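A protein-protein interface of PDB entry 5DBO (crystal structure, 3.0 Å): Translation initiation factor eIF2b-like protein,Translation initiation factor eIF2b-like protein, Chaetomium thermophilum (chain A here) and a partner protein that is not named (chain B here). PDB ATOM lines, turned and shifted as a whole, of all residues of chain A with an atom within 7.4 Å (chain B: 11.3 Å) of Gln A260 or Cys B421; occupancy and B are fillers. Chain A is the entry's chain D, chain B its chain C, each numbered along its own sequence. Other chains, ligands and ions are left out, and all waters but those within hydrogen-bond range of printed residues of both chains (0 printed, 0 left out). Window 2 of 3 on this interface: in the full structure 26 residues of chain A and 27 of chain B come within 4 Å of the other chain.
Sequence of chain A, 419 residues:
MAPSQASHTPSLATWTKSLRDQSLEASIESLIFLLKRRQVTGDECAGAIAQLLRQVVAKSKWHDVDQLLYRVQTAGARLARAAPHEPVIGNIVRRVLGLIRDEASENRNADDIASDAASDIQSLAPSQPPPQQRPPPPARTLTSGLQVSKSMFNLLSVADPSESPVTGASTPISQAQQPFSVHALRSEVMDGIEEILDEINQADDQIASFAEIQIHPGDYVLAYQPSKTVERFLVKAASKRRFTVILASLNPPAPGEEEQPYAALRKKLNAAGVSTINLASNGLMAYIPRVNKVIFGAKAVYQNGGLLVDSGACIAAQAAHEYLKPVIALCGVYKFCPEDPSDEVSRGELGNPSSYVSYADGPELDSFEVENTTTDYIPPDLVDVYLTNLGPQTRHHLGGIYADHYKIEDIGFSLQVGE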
ATOM      1  N   PRO A 252      -5.115 -21.819  15.749  1.00  0.00           N
ATOM      2  CA  PRO A 252      -4.591 -23.002  15.065  1.00  0.00           C
ATOM      3  C   PRO A 252      -5.319 -23.234  13.741  1.00  0.00           C
ATOM      4  O   PRO A 252      -6.458 -22.786  13.588  1.00  0.00           O
ATOM      5  CB  PRO A 252      -4.867 -24.128  16.063  1.00  0.00           C
ATOM      6  CG  PRO A 252      -6.065 -23.658  16.806  1.00  0.00           C
ATOM      7  CD  PRO A 252      -5.847 -22.182  16.975  1.00  0.00           C
ATOM      8  N   PRO A 253      -4.669 -23.921  12.789  1.00  0.00           N
ATOM      9  CA  PRO A 253      -5.322 -24.224  11.513  1.00  0.00           C
ATOM     10  C   PRO A 253      -6.566 -25.090  11.706  1.00  0.00           C
ATOM     11  O   PRO A 253      -6.563 -25.981  12.559  1.00  0.00           O
ATOM     12  CB  PRO A 253      -4.236 -24.971  10.728  1.00  0.00           C
ATOM     13  CG  PRO A 253      -3.286 -25.473  11.766  1.00  0.00           C
ATOM     14  CD  PRO A 253      -3.294 -24.441  12.845  1.00  0.00           C
ATOM     15  N   GLN A 260      -1.190 -26.817   7.673  1.00  0.00           N
ATOM     16  CA  GLN A 260      -0.173 -26.053   8.384  1.00  0.00           C
ATOM     17  C   GLN A 260      -0.050 -24.670   7.755  1.00  0.00           C
ATOM     18  O   GLN A 260      -0.319 -24.504   6.565  1.00  0.00           O
ATOM     19  CB  GLN A 260       1.174 -26.788   8.309  1.00  0.00           C
ATOM     20  CG  GLN A 260       2.081 -26.759   9.547  1.00  0.00           C
ATOM     21  CD  GLN A 260       1.385 -27.118  10.858  1.00  0.00           C
ATOM     22  OE1 GLN A 260       0.768 -26.275  11.510  1.00  0.00           O
ATOM     23  NE2 GLN A 260       1.489 -28.384  11.249  1.00  0.00           N
ATOM     24  N   PRO A 261       0.347 -23.661   8.542  1.00  0.00           N
ATOM     25  CA  PRO A 261       0.264 -22.325   7.954  1.00  0.00           C
ATOM     26  C   PRO A 261       1.592 -21.845   7.365  1.00  0.00           C
ATOM     27  O   PRO A 261       2.660 -22.277   7.805  1.00  0.00           O
ATOM     28  CB  PRO A 261      -0.146 -21.456   9.140  1.00  0.00           C
ATOM     29  CG  PRO A 261       0.438 -22.151  10.334  1.00  0.00           C
ATOM     30  CD  PRO A 261       0.656 -23.607   9.980  1.00  0.00           C
ATOM     31  N   TYR A 262       1.510 -20.951   6.387  1.00  0.00           N
ATOM     32  CA  TYR A 262       2.678 -20.277   5.825  1.00  0.00           C
ATOM     33  C   TYR A 262       3.758 -21.207   5.255  1.00  0.00           C
ATOM     34  O   TYR A 262       4.932 -20.852   5.263  1.00  0.00           O
ATOM     35  CB  TYR A 262       3.315 -19.378   6.894  1.00  0.00           C
ATOM     36  CG  TYR A 262       2.322 -18.600   7.738  1.00  0.00           C
ATOM     37  CD1 TYR A 262       1.549 -17.590   7.181  1.00  0.00           C
ATOM     38  CD2 TYR A 262       2.188 -18.848   9.102  1.00  0.00           C
ATOM     39  CE1 TYR A 262       0.644 -16.872   7.944  1.00  0.00           C
ATOM     40  CE2 TYR A 262       1.286 -18.129   9.877  1.00  0.00           C
ATOM     41  CZ  TYR A 262       0.520 -17.143   9.290  1.00  0.00           C
ATOM     42  OH  TYR A 262      -0.377 -16.422  10.045  1.00  0.00           O
ATOM     43  N   ALA A 263       3.372 -22.375   4.747  1.00  0.00           N
ATOM     44  CA  ALA A 263       4.356 -23.343   4.255  1.00  0.00           C
ATOM     45  C   ALA A 263       5.167 -22.798   3.077  1.00  0.00           C
ATOM     46  O   ALA A 263       6.427 -22.778   3.107  1.00  0.00           O
ATOM     47  CB  ALA A 263       3.655 -24.641   3.854  1.00  0.00           C
ATOM     48  N   ALA A 264       4.432 -22.263   2.101  1.00  0.00           N
ATOM     49  CA  ALA A 264       5.018 -21.709   0.895  1.00  0.00           C
ATOM     50  C   ALA A 264       5.936 -20.585   1.306  1.00  0.00           C
ATOM     51  O   ALA A 264       7.086 -20.529   0.883  1.00  0.00           O
ATOM     52  CB  ALA A 264       3.936 -21.214  -0.059  1.00  0.00           C
ATOM     53  N   ARG A 266       7.285 -20.071   4.366  1.00  0.00           N
ATOM     54  CA  ARG A 266       8.405 -20.395   5.244  1.00  0.00           C
ATOM     55  C   ARG A 266       9.571 -21.088   4.526  1.00  0.00           C
ATOM     56  O   ARG A 266      10.717 -20.758   4.840  1.00  0.00           O
ATOM     57  CB  ARG A 266       7.956 -21.211   6.482  1.00  0.00           C
ATOM     58  CG  ARG A 266       7.378 -22.580   6.234  1.00  0.00           C
ATOM     59  CD  ARG A 266       7.122 -23.319   7.555  1.00  0.00           C
ATOM     60  NE  ARG A 266       6.604 -24.665   7.312  1.00  0.00           N
ATOM     61  CZ  ARG A 266       5.309 -24.966   7.254  1.00  0.00           C
ATOM     62  NH1 ARG A 266       4.401 -24.024   7.486  1.00  0.00           N
ATOM     63  NH2 ARG A 266       4.917 -26.212   7.009  1.00  0.00           N
ATOM     64  N   ILE A 277      10.734 -20.676  12.370  1.00  0.00           N
ATOM     65  CA  ILE A 277      10.056 -21.491  13.366  1.00  0.00           C
ATOM     66  C   ILE A 277       8.630 -20.983  13.522  1.00  0.00           C
ATOM     67  O   ILE A 277       8.413 -19.797  13.769  1.00  0.00           O
ATOM     68  CB  ILE A 277      10.776 -21.468  14.718  1.00  0.00           C
ATOM     69  CG1 ILE A 277       9.842 -21.964  15.818  1.00  0.00           C
ATOM     70  CG2 ILE A 277      11.271 -20.071  15.036  1.00  0.00           C
ATOM     71  CD1 ILE A 277      10.470 -21.949  17.179  1.00  0.00           C
ATOM     72  N   ASN A 278       7.658 -21.873  13.364  1.00  0.00           N
ATOM     73  CA  ASN A 278       6.264 -21.466  13.431  1.00  0.00           C
ATOM     74  C   ASN A 278       5.684 -21.780  14.800  1.00  0.00           C
ATOM     75  O   ASN A 278       5.634 -22.938  15.216  1.00  0.00           O
ATOM     76  CB  ASN A 278       5.445 -22.135  12.328  1.00  0.00           C
ATOM     77  CG  ASN A 278       4.005 -21.656  12.297  1.00  0.00           C
ATOM     78  OD1 ASN A 278       3.676 -20.699  11.598  1.00  0.00           O
ATOM     79  ND2 ASN A 278       3.133 -22.335  13.038  1.00  0.00           N
ATOM     80  N   LEU A 279       5.252 -20.735  15.498  1.00  0.00           N
ATOM     81  CA  LEU A 279       4.759 -20.871  16.857  1.00  0.00           C
ATOM     82  C   LEU A 279       3.293 -21.270  16.888  1.00  0.00           C
ATOM     83  O   LEU A 279       2.431 -20.570  16.352  1.00  0.00           O
ATOM     84  CB  LEU A 279       4.948 -19.559  17.612  1.00  0.00           C
ATOM     85  CG  LEU A 279       6.340 -19.359  18.198  1.00  0.00           C
ATOM     86  CD1 LEU A 279       6.382 -18.099  19.035  1.00  0.00           C
ATOM     87  CD2 LEU A 279       6.734 -20.571  19.023  1.00  0.00           C
ATOM     88  N   ALA A 280       3.013 -22.398  17.530  1.00  0.00           N
ATOM     89  CA  ALA A 280       1.644 -22.836  17.742  1.00  0.00           C
ATOM     90  C   ALA A 280       1.157 -22.392  19.113  1.00  0.00           C
ATOM     91  O   ALA A 280       0.363 -23.077  19.756  1.00  0.00           O
ATOM     92  CB  ALA A 280       1.537 -24.338  17.597  1.00  0.00           C
ATOM     93  N   SER A 281       1.661 -21.254  19.571  1.00  0.00           N
ATOM     94  CA  SER A 281       1.228 -20.699  20.844  1.00  0.00           C
ATOM     95  C   SER A 281       0.372 -19.454  20.645  1.00  0.00           C
ATOM     96  O   SER A 281       0.682 -18.593  19.826  1.00  0.00           O
ATOM     97  CB  SER A 281       2.436 -20.375  21.726  1.00  0.00           C
ATOM     98  OG  SER A 281       2.064 -19.579  22.837  1.00  0.00           O
ATOM     99  N   ALA B 129      12.201 -38.169  19.301  1.00  0.00           N
ATOM    100  CA  ALA B 129      11.310 -37.026  19.451  1.00  0.00           C
ATOM    101  C   ALA B 129      12.117 -35.788  19.794  1.00  0.00           C
ATOM    102  O   ALA B 129      11.786 -34.682  19.370  1.00  0.00           O
ATOM    103  CB  ALA B 129      10.259 -37.294  20.510  1.00  0.00           C
ATOM    104  N   SER B 131      14.995 -35.047  18.747  1.00  0.00           N
ATOM    105  CA  SER B 131      15.544 -34.535  17.498  1.00  0.00           C
ATOM    106  C   SER B 131      14.509 -33.684  16.774  1.00  0.00           C
ATOM    107  O   SER B 131      13.319 -33.994  16.795  1.00  0.00           O
ATOM    108  CB  SER B 131      16.002 -35.678  16.597  1.00  0.00           C
ATOM    109  OG  SER B 131      14.902 -36.467  16.184  1.00  0.00           O
ATOM    110  N   GLY B 132      14.954 -32.607  16.143  1.00  0.00           N
ATOM    111  CA  GLY B 132      14.039 -31.736  15.428  1.00  0.00           C
ATOM    112  C   GLY B 132      13.558 -30.569  16.268  1.00  0.00           C
ATOM    113  O   GLY B 132      12.919 -29.648  15.764  1.00  0.00           O
ATOM    114  N   ILE B 133      13.848 -30.615  17.562  1.00  0.00           N
ATOM    115  CA  ILE B 133      13.566 -29.491  18.441  1.00  0.00           C
ATOM    116  C   ILE B 133      14.539 -28.374  18.099  1.00  0.00           C
ATOM    117  O   ILE B 133      15.735 -28.625  17.980  1.00  0.00           O
ATOM    118  CB  ILE B 133      13.709 -29.894  19.933  1.00  0.00           C
ATOM    119  CG1 ILE B 133      12.660 -30.942  20.306  1.00  0.00           C
ATOM    120  CG2 ILE B 133      13.639 -28.681  20.848  1.00  0.00           C
ATOM    121  CD1 ILE B 133      12.733 -31.371  21.750  1.00  0.00           C
ATOM    122  N   PRO B 134      14.043 -27.136  17.941  1.00  0.00           N
ATOM    123  CA  PRO B 134      14.968 -26.030  17.664  1.00  0.00           C
ATOM    124  C   PRO B 134      16.000 -25.885  18.780  1.00  0.00           C
ATOM    125  O   PRO B 134      15.696 -26.197  19.933  1.00  0.00           O
ATOM    126  CB  PRO B 134      14.042 -24.815  17.592  1.00  0.00           C
ATOM    127  CG  PRO B 134      12.750 -25.385  17.106  1.00  0.00           C
ATOM    128  CD  PRO B 134      12.637 -26.723  17.807  1.00  0.00           C
ATOM    129  N   PHE B 137      15.450 -24.320  22.194  1.00  0.00           N
ATOM    130  CA  PHE B 137      14.609 -25.054  23.127  1.00  0.00           C
ATOM    131  C   PHE B 137      15.064 -26.487  23.418  1.00  0.00           C
ATOM    132  O   PHE B 137      14.313 -27.261  24.010  1.00  0.00           O
ATOM    133  CB  PHE B 137      13.171 -25.063  22.600  1.00  0.00           C
ATOM    134  CG  PHE B 137      12.671 -23.704  22.196  1.00  0.00           C
ATOM    135  CD1 PHE B 137      12.419 -22.738  23.153  1.00  0.00           C
ATOM    136  CD2 PHE B 137      12.472 -23.386  20.862  1.00  0.00           C
ATOM    137  CE1 PHE B 137      11.965 -21.488  22.792  1.00  0.00           C
ATOM    138  CE2 PHE B 137      12.017 -22.135  20.495  1.00  0.00           C
ATOM    139  CZ  PHE B 137      11.764 -21.184  21.461  1.00  0.00           C
ATOM    140  N   MET B 142      10.521 -32.895  27.635  1.00  0.00           N
ATOM    141  CA  MET B 142       9.308 -33.237  26.903  1.00  0.00           C
ATOM    142  C   MET B 142       8.778 -34.600  27.347  1.00  0.00           C
ATOM    143  O   MET B 142       9.550 -35.508  27.639  1.00  0.00           O
ATOM    144  CB  MET B 142       9.593 -33.231  25.397  1.00  0.00           C
ATOM    145  CG  MET B 142       8.470 -33.754  24.515  1.00  0.00           C
ATOM    146  SD  MET B 142       8.861 -33.703  22.746  1.00  0.00           S
ATOM    147  CE  MET B 142      10.549 -34.304  22.730  1.00  0.00           C
ATOM    148  N   TYR B 318      -5.657 -23.510  21.686  1.00  0.00           N
ATOM    149  CA  TYR B 318      -4.960 -24.782  21.523  1.00  0.00           C
ATOM    150  C   TYR B 318      -5.358 -25.797  22.592  1.00  0.00           C
ATOM    151  O   TYR B 318      -5.145 -26.993  22.420  1.00  0.00           O
ATOM    152  CB  TYR B 318      -3.443 -24.567  21.528  1.00  0.00           C
ATOM    153  CG  TYR B 318      -2.931 -23.840  20.297  1.00  0.00           C
ATOM    154  CD1 TYR B 318      -2.483 -24.544  19.186  1.00  0.00           C
ATOM    155  CD2 TYR B 318      -2.917 -22.451  20.241  1.00  0.00           C
ATOM    156  CE1 TYR B 318      -2.024 -23.881  18.057  1.00  0.00           C
ATOM    157  CE2 TYR B 318      -2.458 -21.781  19.121  1.00  0.00           C
ATOM    158  CZ  TYR B 318      -2.014 -22.500  18.032  1.00  0.00           C
ATOM    159  OH  TYR B 318      -1.556 -21.834  16.919  1.00  0.00           O
ATOM    160  N   GLU B 411       8.255 -26.950  29.699  1.00  0.00           N
ATOM    161  CA  GLU B 411       8.021 -28.263  29.100  1.00  0.00           C
ATOM    162  C   GLU B 411       7.474 -28.120  27.674  1.00  0.00           C
ATOM    163  O   GLU B 411       6.575 -27.319  27.421  1.00  0.00           O
ATOM    164  CB  GLU B 411       7.060 -29.085  29.966  1.00  0.00           C
ATOM    165  CG  GLU B 411       6.749 -30.465  29.407  1.00  0.00           C
ATOM    166  CD  GLU B 411       5.761 -31.253  30.262  1.00  0.00           C
ATOM    167  OE1 GLU B 411       5.467 -30.831  31.404  1.00  0.00           O
ATOM    168  OE2 GLU B 411       5.282 -32.306  29.786  1.00  0.00           O
ATOM    169  N   ILE B 412       8.026 -28.890  26.741  1.00  0.00           N
ATOM    170  CA  ILE B 412       7.584 -28.834  25.350  1.00  0.00           C
ATOM    171  C   ILE B 412       6.336 -29.690  25.118  1.00  0.00           C
ATOM    172  O   ILE B 412       6.184 -30.763  25.707  1.00  0.00           O
ATOM    173  CB  ILE B 412       8.708 -29.292  24.389  1.00  0.00           C
ATOM    174  CG1 ILE B 412       9.923 -28.375  24.518  1.00  0.00           C
ATOM    175  CG2 ILE B 412       8.232 -29.296  22.945  1.00  0.00           C
ATOM    176  CD1 ILE B 412      11.036 -28.697  23.558  1.00  0.00           C
ATOM    177  N   ASP B 413       5.446 -29.202  24.258  1.00  0.00           N
ATOM    178  CA  ASP B 413       4.273 -29.952  23.830  1.00  0.00           C
ATOM    179  C   ASP B 413       4.765 -31.144  23.014  1.00  0.00           C
ATOM    180  O   ASP B 413       5.480 -30.971  22.030  1.00  0.00           O
ATOM    181  CB  ASP B 413       3.338 -29.036  23.019  1.00  0.00           C
ATOM    182  CG  ASP B 413       2.018 -29.697  22.627  1.00  0.00           C
ATOM    183  OD1 ASP B 413       1.963 -30.934  22.433  1.00  0.00           O
ATOM    184  OD2 ASP B 413       1.018 -28.950  22.522  1.00  0.00           O
ATOM    185  N   PRO B 414       4.389 -32.361  23.434  1.00  0.00           N
ATOM    186  CA  PRO B 414       4.848 -33.615  22.822  1.00  0.00           C
ATOM    187  C   PRO B 414       4.521 -33.758  21.335  1.00  0.00           C
ATOM    188  O   PRO B 414       5.301 -34.375  20.604  1.00  0.00           O
ATOM    189  CB  PRO B 414       4.109 -34.681  23.636  1.00  0.00           C
ATOM    190  CG  PRO B 414       3.898 -34.044  24.963  1.00  0.00           C
ATOM    191  CD  PRO B 414       3.580 -32.611  24.640  1.00  0.00           C
ATOM    192  N   GLU B 415       3.382 -33.220  20.902  1.00  0.00           N
ATOM    193  CA  GLU B 415       2.973 -33.294  19.496  1.00  0.00           C
ATOM    194  C   GLU B 415       3.586 -32.183  18.626  1.00  0.00           C
ATOM    195  O   GLU B 415       3.763 -32.350  17.416  1.00  0.00           O
ATOM    196  CB  GLU B 415       1.445 -33.258  19.392  1.00  0.00           C
ATOM    197  CG  GLU B 415       0.729 -34.356  20.184  1.00  0.00           C
ATOM    198  CD  GLU B 415       0.771 -35.705  19.485  1.00  0.00           C
ATOM    199  OE1 GLU B 415      -0.147 -36.000  18.688  1.00  0.00           O
ATOM    200  OE2 GLU B 415       1.720 -36.481  19.740  1.00  0.00           O
ATOM    201  N   ARG B 416       3.871 -31.041  19.247  1.00  0.00           N
ATOM    202  CA  ARG B 416       4.416 -29.879  18.546  1.00  0.00           C
ATOM    203  C   ARG B 416       5.905 -29.653  18.810  1.00  0.00           C
ATOM    204  O   ARG B 416       6.353 -28.516  18.921  1.00  0.00           O
ATOM    205  CB  ARG B 416       3.625 -28.631  18.917  1.00  0.00           C
ATOM    206  CG  ARG B 416       2.141 -28.895  19.037  1.00  0.00           C
ATOM    207  CD  ARG B 416       1.360 -27.611  19.089  1.00  0.00           C
ATOM    208  NE  ARG B 416       0.036 -27.816  19.665  1.00  0.00           N
ATOM    209  CZ  ARG B 416      -1.013 -28.263  18.984  1.00  0.00           C
ATOM    210  NH1 ARG B 416      -2.182 -28.417  19.589  1.00  0.00           N
ATOM    211  NH2 ARG B 416      -0.893 -28.550  17.696  1.00  0.00           N
ATOM    212  N   ASN B 417       6.650 -30.737  18.984  1.00  0.00           N
ATOM    213  CA  ASN B 417       8.100 -30.669  19.158  1.00  0.00           C
ATOM    214  C   ASN B 417       8.843 -30.076  17.961  1.00  0.00           C
ATOM    215  O   ASN B 417       9.836 -29.368  18.119  1.00  0.00           O
ATOM    216  CB  ASN B 417       8.645 -32.063  19.458  1.00  0.00           C
ATOM    217  CG  ASN B 417       8.040 -33.122  18.566  1.00  0.00           C
ATOM    218  OD1 ASN B 417       7.097 -32.854  17.821  1.00  0.00           O
ATOM    219  ND2 ASN B 417       8.584 -34.332  18.627  1.00  0.00           N
ATOM    220  N   THR B 418       8.360 -30.394  16.766  1.00  0.00           N
ATOM    221  CA  THR B 418       9.003 -30.018  15.506  1.00  0.00           C
ATOM    222  C   THR B 418       9.107 -28.510  15.261  1.00  0.00           C
ATOM    223  O   THR B 418       8.349 -27.720  15.824  1.00  0.00           O
ATOM    224  CB  THR B 418       8.252 -30.639  14.317  1.00  0.00           C
ATOM    225  OG1 THR B 418       8.781 -30.118  13.093  1.00  0.00           O
ATOM    226  CG2 THR B 418       6.770 -30.304  14.402  1.00  0.00           C
ATOM    227  N   GLY B 419      10.061 -28.126  14.417  1.00  0.00           N
ATOM    228  CA  GLY B 419      10.261 -26.735  14.038  1.00  0.00           C
ATOM    229  C   GLY B 419       9.137 -26.125  13.211  1.00  0.00           C
ATOM    230  O   GLY B 419       8.880 -24.927  13.303  1.00  0.00           O
ATOM    231  N   ASP B 420       8.491 -26.938  12.379  1.00  0.00           N
ATOM    232  CA  ASP B 420       7.359 -26.490  11.568  1.00  0.00           C
ATOM    233  C   ASP B 420       6.170 -26.080  12.421  1.00  0.00           C
ATOM    234  O   ASP B 420       5.441 -25.156  12.075  1.00  0.00           O
ATOM    235  CB  ASP B 420       6.937 -27.570  10.572  1.00  0.00           C
ATOM    236  CG  ASP B 420       7.949 -27.759   9.456  1.00  0.00           C
ATOM    237  OD1 ASP B 420       8.810 -26.868   9.282  1.00  0.00           O
ATOM    238  OD2 ASP B 420       7.875 -28.786   8.747  1.00  0.00           O
ATOM    239  N   CYS B 421       5.936 -26.810  13.500  1.00  0.00           N
ATOM    240  CA  CYS B 421       4.884 -26.461  14.449  1.00  0.00           C
ATOM    241  C   CYS B 421       5.391 -26.598  15.877  1.00  0.00           C
ATOM    242  O   CYS B 421       5.572 -27.711  16.358  1.00  0.00           O
ATOM    243  CB  CYS B 421       3.663 -27.352  14.232  1.00  0.00           C
ATOM    244  SG  CYS B 421       2.271 -27.001  15.300  1.00  0.00           S
ATOM    245  N   PHE B 422       5.600 -25.477  16.562  1.00  0.00           N
ATOM    246  CA  PHE B 422       6.218 -25.520  17.887  1.00  0.00           C
ATOM    247  C   PHE B 422       5.418 -24.811  18.977  1.00  0.00           C
ATOM    248  O   PHE B 422       4.899 -23.714  18.767  1.00  0.00           O
ATOM    249  CB  PHE B 422       7.626 -24.927  17.837  1.00  0.00           C
ATOM    250  CG  PHE B 422       8.381 -25.084  19.124  1.00  0.00           C
ATOM    251  CD1 PHE B 422       9.042 -26.272  19.411  1.00  0.00           C
ATOM    252  CD2 PHE B 422       8.423 -24.055  20.051  1.00  0.00           C
ATOM    253  CE1 PHE B 422       9.730 -26.433  20.598  1.00  0.00           C
ATOM    254  CE2 PHE B 422       9.108 -24.206  21.239  1.00  0.00           C
ATOM    255  CZ  PHE B 422       9.763 -25.399  21.515  1.00  0.00           C
ATOM    256  N   ARG B 423       5.346 -25.434  20.151  1.00  0.00           N
ATOM    257  CA  ARG B 423       4.606 -24.864  21.278  1.00  0.00           C
ATOM    258  C   ARG B 423       5.204 -25.229  22.640  1.00  0.00           C
ATOM    259  O   ARG B 423       5.628 -26.362  22.858  1.00  0.00           O
ATOM    260  CB  ARG B 423       3.142 -25.314  21.234  1.00  0.00           C
ATOM    261  CG  ARG B 423       2.315 -24.776  22.379  1.00  0.00           C
ATOM    262  CD  ARG B 423       0.837 -25.029  22.193  1.00  0.00           C
ATOM    263  NE  ARG B 423       0.054 -24.374  23.241  1.00  0.00           N
ATOM    264  CZ  ARG B 423      -0.413 -24.991  24.319  1.00  0.00           C
ATOM    265  NH1 ARG B 423      -0.189 -26.287  24.492  1.00  0.00           N
ATOM    266  NH2 ARG B 423      -1.114 -24.312  25.218  1.00  0.00           N
ATOM    267  N   LEU B 424       5.208 -24.271  23.562  1.00  0.00           N
ATOM    268  CA  LEU B 424       5.636 -24.521  24.935  1.00  0.00           C
ATOM    269  C   LEU B 424       4.420 -24.525  25.859  1.00  0.00           C
ATOM    270  O   LEU B 424       3.527 -23.689  25.736  1.00  0.00           O
ATOM    271  CB  LEU B 424       6.663 -23.480  25.391  1.00  0.00           C
ATOM    272  CG  LEU B 424       8.044 -23.560  24.735  1.00  0.00           C
ATOM    273  CD1 LEU B 424       8.953 -22.444  25.227  1.00  0.00           C
ATOM    274  CD2 LEU B 424       8.673 -24.916  24.993  1.00  0.00           C
ATOM    275  N   LEU B 425       4.391 -25.488  26.773  1.00  0.00           N
ATOM    276  CA  LEU B 425       3.228 -25.735  27.622  1.00  0.00           C
ATOM    277  C   LEU B 425       2.976 -24.642  28.665  1.00  0.00           C
ATOM    278  O   LEU B 425       1.829 -24.347  29.004  1.00  0.00           O
ATOM    279  CB  LEU B 425       3.382 -27.091  28.312  1.00  0.00           C
ATOM    280  CG  LEU B 425       3.091 -28.320  27.438  1.00  0.00           C
ATOM    281  CD1 LEU B 425       2.886 -29.565  28.294  1.00  0.00           C
ATOM    282  CD2 LEU B 425       1.910 -28.099  26.504  1.00  0.00           C
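The backbone carbonyl oxygen (O) of Gly B419 lies within hydrogen-bond range of the backbone NH (N) of Asn A278, at 3.3 Å.
NE of Arg A266 is in salt-bridge range of OD1 of Asp B420 (3.7 Å).
N of Phe B422 is in hydrogen-bond range of O of Asn A278 (2.9 Å).
N of Ala A280 sits at hydrogen-bond distance from O of Phe B422 (2.6 Å).
The guanidinium group (NE) of Arg B416 lies within salt-bridge range of the side-chain carboxylate (OD2) of Asp B413 (3.2 Å).
OD2 of Asp B413 lies within salt-bridge range of NH1 of Arg B423 (3.5 Å).
N of Arg B423 lies within hydrogen-bond range of O of Arg B416 (3.5 Å).
The side-chain hydroxyl (OG1) of Thr B418 is in hydrogen-bond range of the backbone NH (N) of Asp B420 (3.3 Å).
NH1 of Arg A266 lies within hydrogen-bond range of O of Pro A261.
Pro A252 touches Tyr B318 (CB to CE1, 3.5 Å).
NE2 of Gln A260 touches CB of Cys B421 (3.8 Å).
CE2 of Phe B137 touches CD1 of Ile A277 (3.7 Å).
Asn A278 touches Asp B420.
Cys B421 touches Asn A278 (CA to O, 3.7 Å).
Leu A279 touches Phe B422 (CA to O, 3.4 Å).
CB of Ala A280 touches CD of Arg B416 (3.6 Å).
SG of Cys B421 touches CB of Ala A280 (3.6 Å).
Arg B423 touches Ala A280.
Tyr B318 touches Ser A281 (CE2 to C, 3.97 Å).
No residue of chain B comes within 4 Å of Pro A261.
Asn A278 touches four residues of chain B.
Of the printed residues of chain A, Tyr B318 touches Pro A252 (3.5 Å), Ala A280 (3.0 Å) and Ser A281 (3.97 Å).
Asn B417 touches none of the printed residues of chain A.
Of the printed residues of chain A, Asp B420 touches Arg A266 (3.7 Å) and Asn A278 (3.0 Å).
Cys B421 touches just these residues of chain A: Gln A260 (3.8 Å), Asn A278 (3.7 Å) and Ala A280 (3.6 Å).
The nearest residue of chain B that does not touch Gln A260 is Asp B420 (4.5 Å).
The nearest residue of chain A that does not touch Cys B421 is Leu A279 (5.8 Å).
Printed residues of chain A that touch a printed residue of chain B: Pro A252, Gln A260, Arg A266, Ile A277, Asn A278, Leu A279, Ala A280 and Ser A281.
Hydrophobic or aromatic side chains of chain B within 4 Å of the printed part of chain A: Phe B137, Tyr B318 and Phe B422.
Among the printed residues, Asp or Glu carboxylates within 4 Å of a Lys or Arg side-chain nitrogen of the other chain: Arg A266 with Asp B420.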
